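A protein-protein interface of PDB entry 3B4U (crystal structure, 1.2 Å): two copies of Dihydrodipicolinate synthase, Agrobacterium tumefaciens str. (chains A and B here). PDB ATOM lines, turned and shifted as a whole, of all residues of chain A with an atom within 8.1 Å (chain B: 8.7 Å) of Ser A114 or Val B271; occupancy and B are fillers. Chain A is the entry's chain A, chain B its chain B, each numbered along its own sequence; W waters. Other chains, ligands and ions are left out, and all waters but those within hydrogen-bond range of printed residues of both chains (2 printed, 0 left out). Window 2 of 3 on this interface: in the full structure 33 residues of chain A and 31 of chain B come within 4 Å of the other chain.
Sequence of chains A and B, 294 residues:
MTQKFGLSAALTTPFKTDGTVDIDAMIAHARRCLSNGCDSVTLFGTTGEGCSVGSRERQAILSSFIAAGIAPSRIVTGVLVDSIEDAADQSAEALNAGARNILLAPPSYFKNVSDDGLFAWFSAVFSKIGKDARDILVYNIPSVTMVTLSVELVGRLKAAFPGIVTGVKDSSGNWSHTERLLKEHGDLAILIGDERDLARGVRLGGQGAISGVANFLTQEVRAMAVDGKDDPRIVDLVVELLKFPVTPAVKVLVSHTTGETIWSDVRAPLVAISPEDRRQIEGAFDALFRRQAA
Of the printed residues of chain B, Phe A110 touches Leu B270 (3.7 Å).
Of the printed residues of chain B, Gly A117 touches Ala B268 (3.5 Å), Pro B269 (3.3 Å) and Val B271 (3.6 Å).
Of the printed residues of chain B, Ala A120 touches Ala B268.
Printed residues of chain B within 4 Å of Trp A121: Ala B268.
Asp B265 touches none of the printed residues of chain A.
Printed residues of chain A within 4 Å of Pro B269: Gly A117 (3.3 Å).
Val B271 touches two residues of chain A.
No residue of chain A comes within 4 Å of Ala B272.
The nearest residue of chain B that does not touch Ser A114 is Pro B269 (4.6 Å).
The nearest residue of chain A that does not touch Val B271 is Asp A116 (4.3 Å).
No position is printed for both chains.
Of the 7 pairs that touch across the chains among the printed residues, none has its exchanged pair printed and touching as well.
Water W1 lies within hydrogen-bond range of O of Pro B269 (2.7 Å) and N of Ser A114 (2.9 Å).
Water W2 lies within hydrogen-bond range of the backbone carbonyl oxygen (O) of Ala B268 and the indole nitrogen (NE1) of Trp A121.
OG of Ser A114 is in hydrogen-bond range of N of Gly A117 (3.0 Å).
Of the 20 printed residues of chain B, 4 touch a printed residue of chain A.
Hydrophobic or aromatic side chains of chain B within 4 Å of the printed part of chain A: Ala B268, Leu B270 and Val B271.
Of the 18 printed residues of chain A, 5 touch a printed residue of chain B.
CE2 of Phe A110 touches CD1 of Leu B270 (3.7 Å).
Val B271 touches Ser A114.
Gly A117 touches Ala B268.
Gly A117 touches Pro B269.
N of Gly A117 touches CG1 of Val B271, at 3.6 Å.
CB of Ala B268 touches C of Ala A120, at 3.8 Å.
Ala B268 touches Trp A121.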
ATOM      1  N   PHE A 110     -29.564  -4.150  -2.880  1.00  0.00           N
ATOM      2  CA  PHE A 110     -29.842  -5.532  -3.208  1.00  0.00           C
ATOM      3  C   PHE A 110     -28.798  -6.449  -2.570  1.00  0.00           C
ATOM      4  O   PHE A 110     -27.592  -6.154  -2.519  1.00  0.00           O
ATOM      5  CB  PHE A 110     -29.883  -5.755  -4.727  1.00  0.00           C
ATOM      6  CG  PHE A 110     -31.098  -5.171  -5.431  1.00  0.00           C
ATOM      7  CD1 PHE A 110     -32.375  -5.401  -4.960  1.00  0.00           C
ATOM      8  CD2 PHE A 110     -30.970  -4.445  -6.607  1.00  0.00           C
ATOM      9  CE1 PHE A 110     -33.504  -4.922  -5.652  1.00  0.00           C
ATOM     10  CE2 PHE A 110     -32.072  -3.979  -7.283  1.00  0.00           C
ATOM     11  CZ  PHE A 110     -33.344  -4.192  -6.792  1.00  0.00           C
ATOM     12  N   LYS A 111     -29.272  -7.595  -2.088  1.00  0.00           N
ATOM     13  CA  LYS A 111     -28.449  -8.575  -1.390  1.00  0.00           C
ATOM     14  C   LYS A 111     -28.209  -9.784  -2.281  1.00  0.00           C
ATOM     15  O   LYS A 111     -28.939 -10.040  -3.209  1.00  0.00           O
ATOM     16  CB  LYS A 111     -29.170  -9.025  -0.096  1.00  0.00           C
ATOM     17  CG  LYS A 111     -29.415  -7.883   0.909  1.00  0.00           C
ATOM     18  CD  LYS A 111     -28.134  -7.475   1.555  1.00  0.00           C
ATOM     19  CE  LYS A 111     -28.245  -6.240   2.440  1.00  0.00           C
ATOM     20  NZ  LYS A 111     -28.486  -4.939   1.704  1.00  0.00           N
ATOM     21  N   ASN A 112     -27.166 -10.525  -1.945  1.00  0.00           N
ATOM     22  CA  ASN A 112     -26.857 -11.786  -2.638  1.00  0.00           C
ATOM     23  C   ASN A 112     -26.730 -11.609  -4.119  1.00  0.00           C
ATOM     24  O   ASN A 112     -27.268 -12.395  -4.902  1.00  0.00           O
ATOM     25  CB  ASN A 112     -27.921 -12.851  -2.352  1.00  0.00           C
ATOM     26  CG  ASN A 112     -28.093 -13.107  -0.903  1.00  0.00           C
ATOM     27  OD1 ASN A 112     -29.153 -12.817  -0.333  1.00  0.00           O
ATOM     28  ND2 ASN A 112     -27.040 -13.581  -0.263  1.00  0.00           N
ATOM     29  N   VAL A 113     -25.985 -10.594  -4.527  1.00  0.00           N
ATOM     30  CA  VAL A 113     -25.808 -10.324  -5.944  1.00  0.00           C
ATOM     31  C   VAL A 113     -24.617 -11.126  -6.470  1.00  0.00           C
ATOM     32  O   VAL A 113     -23.704 -11.490  -5.731  1.00  0.00           O
ATOM     33  CB  VAL A 113     -25.646  -8.815  -6.221  1.00  0.00           C
ATOM     34  CG1 VAL A 113     -26.981  -8.092  -5.854  1.00  0.00           C
ATOM     35  CG2 VAL A 113     -24.448  -8.194  -5.497  1.00  0.00           C
ATOM     36  N   SER A 114     -24.646 -11.406  -7.760  1.00  0.00           N
ATOM     37  CA  SER A 114     -23.648 -12.252  -8.401  1.00  0.00           C
ATOM     38  C   SER A 114     -22.402 -11.486  -8.813  1.00  0.00           C
ATOM     39  O   SER A 114     -22.424 -10.274  -9.062  1.00  0.00           O
ATOM     40  CB  SER A 114     -24.259 -12.940  -9.629  1.00  0.00           C
ATOM     41  OG  SER A 114     -24.518 -11.980 -10.638  1.00  0.00           O
ATOM     42  N   ASP A 115     -21.296 -12.211  -8.986  1.00  0.00           N
ATOM     43  CA  ASP A 115     -20.106 -11.627  -9.575  1.00  0.00           C
ATOM     44  C   ASP A 115     -20.380 -11.017 -10.943  1.00  0.00           C
ATOM     45  O   ASP A 115     -19.871  -9.949 -11.251  1.00  0.00           O
ATOM     46  CB  ASP A 115     -19.003 -12.679  -9.748  1.00  0.00           C
ATOM     47  CG  ASP A 115     -18.291 -13.020  -8.471  1.00  0.00           C
ATOM     48  OD1 ASP A 115     -18.805 -12.719  -7.384  1.00  0.00           O
ATOM     49  OD2 ASP A 115     -17.194 -13.605  -8.574  1.00  0.00           O
ATOM     50  N   ASP A 116     -21.174 -11.685 -11.777  1.00  0.00           N
ATOM     51  CA  ASP A 116     -21.492 -11.172 -13.107  1.00  0.00           C
ATOM     52  C   ASP A 116     -22.227  -9.829 -12.989  1.00  0.00           C
ATOM     53  O   ASP A 116     -21.929  -8.882 -13.703  1.00  0.00           O
ATOM     54  CB  ASP A 116     -22.336 -12.196 -13.870  1.00  0.00           C
ATOM     55  CG  ASP A 116     -21.555 -13.374 -14.381  1.00  0.00           C
ATOM     56  OD1 ASP A 116     -20.315 -13.349 -14.332  1.00  0.00           O
ATOM     57  OD2 ASP A 116     -22.215 -14.322 -14.852  1.00  0.00           O
ATOM     58  N   GLY A 117     -23.175  -9.728 -12.053  1.00  0.00           N
ATOM     59  CA  GLY A 117     -23.895  -8.473 -11.878  1.00  0.00           C
ATOM     60  C   GLY A 117     -22.984  -7.357 -11.392  1.00  0.00           C
ATOM     61  O   GLY A 117     -23.100  -6.219 -11.817  1.00  0.00           O
ATOM     62  N   LEU A 118     -22.063  -7.699 -10.506  1.00  0.00           N
ATOM     63  CA  LEU A 118     -21.099  -6.721 -10.020  1.00  0.00           C
ATOM     64  C   LEU A 118     -20.148  -6.274 -11.123  1.00  0.00           C
ATOM     65  O   LEU A 118     -19.859  -5.101 -11.248  1.00  0.00           O
ATOM     66  CB  LEU A 118     -20.305  -7.252  -8.839  1.00  0.00           C
ATOM     67  CG  LEU A 118     -21.143  -7.454  -7.583  1.00  0.00           C
ATOM     68  CD1 LEU A 118     -20.360  -8.240  -6.547  1.00  0.00           C
ATOM     69  CD2 LEU A 118     -21.614  -6.091  -7.004  1.00  0.00           C
ATOM     70  N   PHE A 119     -19.637  -7.213 -11.932  1.00  0.00           N
ATOM     71  CA  PHE A 119     -18.772  -6.835 -13.041  1.00  0.00           C
ATOM     72  C   PHE A 119     -19.507  -5.851 -13.965  1.00  0.00           C
ATOM     73  O   PHE A 119     -18.963  -4.822 -14.343  1.00  0.00           O
ATOM     74  CB  PHE A 119     -18.333  -8.071 -13.829  1.00  0.00           C
ATOM     75  CG  PHE A 119     -17.462  -7.698 -15.006  1.00  0.00           C
ATOM     76  CD1 PHE A 119     -16.112  -7.473 -14.834  1.00  0.00           C
ATOM     77  CD2 PHE A 119     -18.019  -7.465 -16.262  1.00  0.00           C
ATOM     78  CE1 PHE A 119     -15.330  -7.063 -15.890  1.00  0.00           C
ATOM     79  CE2 PHE A 119     -17.253  -7.026 -17.315  1.00  0.00           C
ATOM     80  CZ  PHE A 119     -15.907  -6.831 -17.114  1.00  0.00           C
ATOM     81  N   ALA A 120     -20.772  -6.156 -14.292  1.00  0.00           N
ATOM     82  CA  ALA A 120     -21.567  -5.298 -15.162  1.00  0.00           C
ATOM     83  C   ALA A 120     -21.790  -3.917 -14.522  1.00  0.00           C
ATOM     84  O   ALA A 120     -21.749  -2.901 -15.208  1.00  0.00           O
ATOM     85  CB  ALA A 120     -22.901  -5.971 -15.487  1.00  0.00           C
ATOM     86  N   TRP A 121     -21.940  -3.863 -13.198  1.00  0.00           N
ATOM     87  CA  TRP A 121     -22.176  -2.595 -12.510  1.00  0.00           C
ATOM     88  C   TRP A 121     -20.926  -1.717 -12.590  1.00  0.00           C
ATOM     89  O   TRP A 121     -20.977  -0.555 -12.998  1.00  0.00           O
ATOM     90  CB  TRP A 121     -22.564  -2.826 -11.051  1.00  0.00           C
ATOM     91  CG  TRP A 121     -23.002  -1.596 -10.354  1.00  0.00           C
ATOM     92  CD1 TRP A 121     -24.266  -1.099 -10.314  1.00  0.00           C
ATOM     93  CD2 TRP A 121     -22.196  -0.704  -9.559  1.00  0.00           C
ATOM     94  NE1 TRP A 121     -24.313   0.033  -9.540  1.00  0.00           N
ATOM     95  CE2 TRP A 121     -23.055   0.302  -9.079  1.00  0.00           C
ATOM     96  CE3 TRP A 121     -20.858  -0.675  -9.180  1.00  0.00           C
ATOM     97  CZ2 TRP A 121     -22.609   1.307  -8.246  1.00  0.00           C
ATOM     98  CZ3 TRP A 121     -20.420   0.317  -8.351  1.00  0.00           C
ATOM     99  CH2 TRP A 121     -21.291   1.293  -7.883  1.00  0.00           C
ATOM    100  N   VAL A 147     -21.609  -7.369   0.474  1.00  0.00           N
ATOM    101  CA  VAL A 147     -21.198  -7.659  -0.901  1.00  0.00           C
ATOM    102  C   VAL A 147     -19.701  -7.913  -0.887  1.00  0.00           C
ATOM    103  O   VAL A 147     -18.902  -7.032  -0.715  1.00  0.00           O
ATOM    104  CB  VAL A 147     -21.559  -6.507  -1.853  1.00  0.00           C
ATOM    105  CG1 VAL A 147     -21.150  -6.904  -3.263  1.00  0.00           C
ATOM    106  CG2 VAL A 147     -23.051  -6.191  -1.798  1.00  0.00           C
ATOM    107  N   THR A 148     -19.322  -9.153  -1.060  1.00  0.00           N
ATOM    108  CA  THR A 148     -17.946  -9.545  -1.171  1.00  0.00           C
ATOM    109  C   THR A 148     -17.506  -9.385  -2.611  1.00  0.00           C
ATOM    110  O   THR A 148     -18.242  -9.702  -3.538  1.00  0.00           O
ATOM    111  CB  THR A 148     -17.815 -11.019  -0.747  1.00  0.00           C
ATOM    112  OG1 THR A 148     -18.262 -11.154   0.612  1.00  0.00           O
ATOM    113  CG2 THR A 148     -16.393 -11.522  -0.946  1.00  0.00           C
ATOM    114  N   LEU A 149     -16.332  -8.805  -2.767  1.00  0.00           N
ATOM    115  CA  LEU A 149     -15.663  -8.733  -4.064  1.00  0.00           C
ATOM    116  C   LEU A 149     -14.706  -9.902  -4.158  1.00  0.00           C
ATOM    117  O   LEU A 149     -13.647  -9.906  -3.541  1.00  0.00           O
ATOM    118  CB  LEU A 149     -14.927  -7.398  -4.224  1.00  0.00           C
ATOM    119  CG  LEU A 149     -15.774  -6.130  -4.021  1.00  0.00           C
ATOM    120  CD1 LEU A 149     -14.927  -4.893  -4.238  1.00  0.00           C
ATOM    121  CD2 LEU A 149     -17.030  -6.125  -4.889  1.00  0.00           C
ATOM    122  N   SER A 150     -15.078 -10.917  -4.916  1.00  0.00           N
ATOM    123  CA  SER A 150     -14.282 -12.112  -4.969  1.00  0.00           C
ATOM    124  C   SER A 150     -12.945 -11.870  -5.663  1.00  0.00           C
ATOM    125  O   SER A 150     -12.772 -10.938  -6.431  1.00  0.00           O
ATOM    126  CB  SER A 150     -15.036 -13.222  -5.707  1.00  0.00           C
ATOM    127  OG  SER A 150     -15.117 -12.922  -7.107  1.00  0.00           O
ATOM    128  N   LEU A 153     -13.577 -11.856  -9.293  1.00  0.00           N
ATOM    129  CA  LEU A 153     -14.126 -10.600  -9.776  1.00  0.00           C
ATOM    130  C   LEU A 153     -13.036  -9.560  -9.897  1.00  0.00           C
ATOM    131  O   LEU A 153     -12.974  -8.837 -10.884  1.00  0.00           O
ATOM    132  CB  LEU A 153     -15.256 -10.112  -8.849  1.00  0.00           C
ATOM    133  CG  LEU A 153     -15.760  -8.719  -9.219  1.00  0.00           C
ATOM    134  CD1 LEU A 153     -16.437  -8.695 -10.604  1.00  0.00           C
ATOM    135  CD2 LEU A 153     -16.710  -8.225  -8.156  1.00  0.00           C
ATOM    136  N   ARG A 156     -11.214 -10.120 -13.051  1.00  0.00           N
ATOM    137  CA  ARG A 156     -11.981  -9.672 -14.202  1.00  0.00           C
ATOM    138  C   ARG A 156     -11.913  -8.188 -14.341  1.00  0.00           C
ATOM    139  O   ARG A 156     -11.817  -7.662 -15.456  1.00  0.00           O
ATOM    140  CB  ARG A 156     -13.428 -10.172 -14.143  1.00  0.00           C
ATOM    141  CG  ARG A 156     -13.542 -11.684 -14.269  1.00  0.00           C
ATOM    142  CD  ARG A 156     -14.894 -12.210 -13.861  1.00  0.00           C
ATOM    143  NE  ARG A 156     -15.933 -11.793 -14.798  1.00  0.00           N
ATOM    144  CZ  ARG A 156     -17.226 -12.032 -14.635  1.00  0.00           C
ATOM    145  NH1 ARG A 156     -17.671 -12.568 -13.525  1.00  0.00           N
ATOM    146  NH2 ARG A 156     -18.084 -11.714 -15.585  1.00  0.00           N
ATOM    147  N   GLU B  49     -36.447  -1.431  -8.917  1.00  0.00           N
ATOM    148  CA  GLU B  49     -35.013  -1.251  -8.959  1.00  0.00           C
ATOM    149  C   GLU B  49     -34.651   0.191  -8.623  1.00  0.00           C
ATOM    150  O   GLU B  49     -33.700   0.772  -9.135  1.00  0.00           O
ATOM    151  CB  GLU B  49     -34.414  -1.685 -10.304  1.00  0.00           C
ATOM    152  CG  GLU B  49     -34.609  -3.153 -10.570  1.00  0.00           C
ATOM    153  CD  GLU B  49     -34.335  -3.517 -12.005  1.00  0.00           C
ATOM    154  OE1 GLU B  49     -33.139  -3.572 -12.377  1.00  0.00           O
ATOM    155  OE2 GLU B  49     -35.313  -3.775 -12.747  1.00  0.00           O
ATOM    156  N   PHE B 244     -36.127 -18.177  -7.731  1.00  0.00           N
ATOM    157  CA  PHE B 244     -35.551 -17.190  -8.669  1.00  0.00           C
ATOM    158  C   PHE B 244     -35.430 -15.819  -7.988  1.00  0.00           C
ATOM    159  O   PHE B 244     -36.228 -15.490  -7.109  1.00  0.00           O
ATOM    160  CB  PHE B 244     -36.439 -17.121  -9.930  1.00  0.00           C
ATOM    161  CG  PHE B 244     -36.845 -18.472 -10.476  1.00  0.00           C
ATOM    162  CD1 PHE B 244     -35.947 -19.238 -11.216  1.00  0.00           C
ATOM    163  CD2 PHE B 244     -38.114 -18.977 -10.264  1.00  0.00           C
ATOM    164  CE1 PHE B 244     -36.323 -20.494 -11.703  1.00  0.00           C
ATOM    165  CE2 PHE B 244     -38.489 -20.231 -10.747  1.00  0.00           C
ATOM    166  CZ  PHE B 244     -37.592 -20.983 -11.469  1.00  0.00           C
ATOM    167  N   PRO B 245     -34.433 -14.975  -8.374  1.00  0.00           N
ATOM    168  CA  PRO B 245     -34.403 -13.599  -7.848  1.00  0.00           C
ATOM    169  C   PRO B 245     -35.724 -12.873  -8.077  1.00  0.00           C
ATOM    170  O   PRO B 245     -36.291 -12.958  -9.148  1.00  0.00           O
ATOM    171  CB  PRO B 245     -33.235 -12.942  -8.624  1.00  0.00           C
ATOM    172  CG  PRO B 245     -32.301 -14.065  -8.773  1.00  0.00           C
ATOM    173  CD  PRO B 245     -33.240 -15.204  -9.213  1.00  0.00           C
ATOM    174  N   VAL B 246     -36.213 -12.203  -7.050  1.00  0.00           N
ATOM    175  CA  VAL B 246     -37.623 -11.793  -7.040  1.00  0.00           C
ATOM    176  C   VAL B 246     -37.952 -10.764  -8.120  1.00  0.00           C
ATOM    177  O   VAL B 246     -38.911 -10.941  -8.879  1.00  0.00           O
ATOM    178  CB  VAL B 246     -38.069 -11.270  -5.630  1.00  0.00           C
ATOM    179  CG1 VAL B 246     -39.537 -10.922  -5.608  1.00  0.00           C
ATOM    180  CG2 VAL B 246     -37.760 -12.239  -4.506  1.00  0.00           C
ATOM    181  N   THR B 247     -37.186  -9.685  -8.190  1.00  0.00           N
ATOM    182  CA  THR B 247     -37.517  -8.626  -9.107  1.00  0.00           C
ATOM    183  C   THR B 247     -37.345  -9.047 -10.570  1.00  0.00           C
ATOM    184  O   THR B 247     -38.243  -8.836 -11.395  1.00  0.00           O
ATOM    185  CB  THR B 247     -36.761  -7.341  -8.724  1.00  0.00           C
ATOM    186  OG1 THR B 247     -37.197  -6.942  -7.406  1.00  0.00           O
ATOM    187  CG2 THR B 247     -37.027  -6.222  -9.734  1.00  0.00           C
ATOM    188  N   PRO B 248     -36.221  -9.704 -10.913  1.00  0.00           N
ATOM    189  CA  PRO B 248     -36.123 -10.205 -12.283  1.00  0.00           C
ATOM    190  C   PRO B 248     -37.274 -11.175 -12.671  1.00  0.00           C
ATOM    191  O   PRO B 248     -37.762 -11.130 -13.794  1.00  0.00           O
ATOM    192  CB  PRO B 248     -34.738 -10.864 -12.305  1.00  0.00           C
ATOM    193  CG  PRO B 248     -33.930 -10.113 -11.243  1.00  0.00           C
ATOM    194  CD  PRO B 248     -34.961  -9.888 -10.164  1.00  0.00           C
ATOM    195  N   ALA B 249     -37.727 -12.017 -11.743  1.00  0.00           N
ATOM    196  CA  ALA B 249     -38.836 -12.926 -12.032  1.00  0.00           C
ATOM    197  C   ALA B 249     -40.167 -12.210 -12.227  1.00  0.00           C
ATOM    198  O   ALA B 249     -40.944 -12.560 -13.100  1.00  0.00           O
ATOM    199  CB  ALA B 249     -38.951 -14.003 -10.959  1.00  0.00           C
ATOM    200  N   LYS B 251     -40.440  -9.253 -13.468  1.00  0.00           N
ATOM    201  CA  LYS B 251     -40.332  -8.684 -14.811  1.00  0.00           C
ATOM    202  C   LYS B 251     -40.581  -9.709 -15.920  1.00  0.00           C
ATOM    203  O   LYS B 251     -41.230  -9.404 -16.919  1.00  0.00           O
ATOM    204  CB  LYS B 251     -38.992  -7.977 -14.965  1.00  0.00           C
ATOM    205  CG  LYS B 251     -38.894  -6.678 -14.145  1.00  0.00           C
ATOM    206  CD  LYS B 251     -37.523  -5.993 -14.308  1.00  0.00           C
ATOM    207  CE  LYS B 251     -37.654  -4.719 -15.115  1.00  0.00           C
ATOM    208  NZ  LYS B 251     -36.345  -4.043 -15.255  1.00  0.00           N
ATOM    209  N   VAL B 252     -40.107 -10.935 -15.718  1.00  0.00           N
ATOM    210  CA  VAL B 252     -40.402 -12.017 -16.670  1.00  0.00           C
ATOM    211  C   VAL B 252     -41.918 -12.178 -16.835  1.00  0.00           C
ATOM    212  O   VAL B 252     -42.408 -12.347 -17.927  1.00  0.00           O
ATOM    213  CB  VAL B 252     -39.760 -13.356 -16.186  1.00  0.00           C
ATOM    214  CG1 VAL B 252     -40.345 -14.556 -16.913  1.00  0.00           C
ATOM    215  CG2 VAL B 252     -38.252 -13.365 -16.322  1.00  0.00           C
ATOM    216  N   SER B 264     -37.602  -7.882 -19.907  1.00  0.00           N
ATOM    217  CA  SER B 264     -36.557  -8.878 -19.669  1.00  0.00           C
ATOM    218  C   SER B 264     -35.420  -8.246 -18.891  1.00  0.00           C
ATOM    219  O   SER B 264     -35.085  -8.712 -17.760  1.00  0.00           O
ATOM    220  CB  SER B 264     -36.117  -9.577 -20.983  1.00  0.00           C
ATOM    221  OG  SER B 264     -35.869  -8.642 -22.017  1.00  0.00           O
ATOM    222  N   ASP B 265     -34.946  -7.146 -19.461  1.00  0.00           N
ATOM    223  CA  ASP B 265     -33.724  -6.501 -19.043  1.00  0.00           C
ATOM    224  C   ASP B 265     -33.818  -5.933 -17.627  1.00  0.00           C
ATOM    225  O   ASP B 265     -34.811  -5.292 -17.249  1.00  0.00           O
ATOM    226  CB  ASP B 265     -33.326  -5.389 -20.027  1.00  0.00           C
ATOM    227  CG  ASP B 265     -32.676  -5.915 -21.299  1.00  0.00           C
ATOM    228  OD1 ASP B 265     -32.449  -7.131 -21.380  1.00  0.00           O
ATOM    229  OD2 ASP B 265     -32.441  -5.092 -22.202  1.00  0.00           O
ATOM    230  N   VAL B 266     -32.761  -6.167 -16.864  1.00  0.00           N
ATOM    231  CA  VAL B 266     -32.608  -5.600 -15.544  1.00  0.00           C
ATOM    232  C   VAL B 266     -31.323  -4.827 -15.505  1.00  0.00           C
ATOM    233  O   VAL B 266     -30.431  -5.019 -16.336  1.00  0.00           O
ATOM    234  CB  VAL B 266     -32.592  -6.688 -14.437  1.00  0.00           C
ATOM    235  CG1 VAL B 266     -33.975  -7.354 -14.336  1.00  0.00           C
ATOM    236  CG2 VAL B 266     -31.484  -7.718 -14.653  1.00  0.00           C
ATOM    237  N   ARG B 267     -31.190  -3.959 -14.530  1.00  0.00           N
ATOM    238  CA  ARG B 267     -29.984  -3.184 -14.356  1.00  0.00           C
ATOM    239  C   ARG B 267     -29.052  -3.877 -13.384  1.00  0.00           C
ATOM    240  O   ARG B 267     -29.462  -4.437 -12.368  1.00  0.00           O
ATOM    241  CB  ARG B 267     -30.333  -1.768 -13.856  1.00  0.00           C
ATOM    242  CG  ARG B 267     -29.263  -0.758 -13.790  1.00  0.00           C
ATOM    243  CD  ARG B 267     -29.874   0.643 -13.752  1.00  0.00           C
ATOM    244  NE  ARG B 267     -30.236   1.314 -15.012  1.00  0.00           N
ATOM    245  CZ  ARG B 267     -30.625   2.608 -15.046  1.00  0.00           C
ATOM    246  NH1 ARG B 267     -30.776   3.263 -13.913  1.00  0.00           N
ATOM    247  NH2 ARG B 267     -30.888   3.260 -16.176  1.00  0.00           N
ATOM    248  N   ALA B 268     -27.763  -3.840 -13.679  1.00  0.00           N
ATOM    249  CA  ALA B 268     -26.758  -4.320 -12.753  1.00  0.00           C
ATOM    250  C   ALA B 268     -26.989  -3.604 -11.414  1.00  0.00           C
ATOM    251  O   ALA B 268     -27.326  -2.434 -11.391  1.00  0.00           O
ATOM    252  CB  ALA B 268     -25.359  -4.001 -13.310  1.00  0.00           C
ATOM    253  N   PRO B 269     -26.787  -4.299 -10.285  1.00  0.00           N
ATOM    254  CA  PRO B 269     -26.159  -5.604 -10.143  1.00  0.00           C
ATOM    255  C   PRO B 269     -27.058  -6.834 -10.262  1.00  0.00           C
ATOM    256  O   PRO B 269     -26.588  -7.953 -10.032  1.00  0.00           O
ATOM    257  CB  PRO B 269     -25.610  -5.501  -8.729  1.00  0.00           C
ATOM    258  CG  PRO B 269     -26.670  -4.728  -8.028  1.00  0.00           C
ATOM    259  CD  PRO B 269     -27.072  -3.688  -8.978  1.00  0.00           C
ATOM    260  N   LEU B 270     -28.317  -6.655 -10.638  1.00  0.00           N
ATOM    261  CA  LEU B 270     -29.165  -7.785 -10.999  1.00  0.00           C
ATOM    262  C   LEU B 270     -28.710  -8.341 -12.343  1.00  0.00           C
ATOM    263  O   LEU B 270     -28.048  -7.640 -13.110  1.00  0.00           O
ATOM    264  CB  LEU B 270     -30.629  -7.371 -11.048  1.00  0.00           C
ATOM    265  CG  LEU B 270     -31.238  -6.785  -9.769  1.00  0.00           C
ATOM    266  CD1 LEU B 270     -32.695  -6.476  -9.944  1.00  0.00           C
ATOM    267  CD2 LEU B 270     -31.033  -7.720  -8.573  1.00  0.00           C
ATOM    268  N   VAL B 271     -29.090  -9.584 -12.595  1.00  0.00           N
ATOM    269  CA  VAL B 271     -28.847 -10.221 -13.882  1.00  0.00           C
ATOM    270  C   VAL B 271     -30.138 -10.807 -14.442  1.00  0.00           C
ATOM    271  O   VAL B 271     -31.031 -11.133 -13.716  1.00  0.00           O
ATOM    272  CB  VAL B 271     -27.734 -11.281 -13.786  1.00  0.00           C
ATOM    273  CG1 VAL B 271     -26.398 -10.620 -13.340  1.00  0.00           C
ATOM    274  CG2 VAL B 271     -28.102 -12.419 -12.928  1.00  0.00           C
ATOM    275  N   ALA B 272     -30.176 -10.896 -15.769  1.00  0.00           N
ATOM    276  CA  ALA B 272     -31.261 -11.472 -16.549  1.00  0.00           C
ATOM    277  C   ALA B 272     -31.609 -12.880 -16.088  1.00  0.00           C
ATOM    278  O   ALA B 272     -30.739 -13.653 -15.819  1.00  0.00           O
ATOM    279  CB  ALA B 272     -30.830 -11.504 -18.049  1.00  0.00           C
ATOM    280  N   ILE B 273     -32.892 -13.214 -16.000  1.00  0.00           N
ATOM    281  CA  ILE B 273     -33.317 -14.610 -15.878  1.00  0.00           C
ATOM    282  C   ILE B 273     -32.955 -15.363 -17.173  1.00  0.00           C
ATOM    283  O   ILE B 273     -33.244 -14.904 -18.253  1.00  0.00           O
ATOM    284  CB  ILE B 273     -34.846 -14.688 -15.656  1.00  0.00           C
ATOM    285  CG1 ILE B 273     -35.274 -13.983 -14.355  1.00  0.00           C
ATOM    286  CG2 ILE B 273     -35.323 -16.145 -15.673  1.00  0.00           C
ATOM    287  CD1 ILE B 273     -34.816 -14.647 -13.124  1.00  0.00           C
ATOM    288  N   SER B 274     -32.357 -16.547 -17.050  1.00  0.00           N
ATOM    289  CA  SER B 274     -31.983 -17.345 -18.240  1.00  0.00           C
ATOM    290  C   SER B 274     -33.204 -17.890 -19.002  1.00  0.00           C
ATOM    291  O   SER B 274     -34.294 -17.987 -18.414  1.00  0.00           O
ATOM    292  CB  SER B 274     -31.128 -18.532 -17.841  1.00  0.00           C
ATOM    293  OG  SER B 274     -31.965 -19.557 -17.318  1.00  0.00           O
HETATM  294  O   HOH W   1     -26.829 -10.567  -9.429  1.00  0.00           O
HETATM  295  O   HOH W   2     -27.205  -0.004 -10.006  1.00  0.00           O
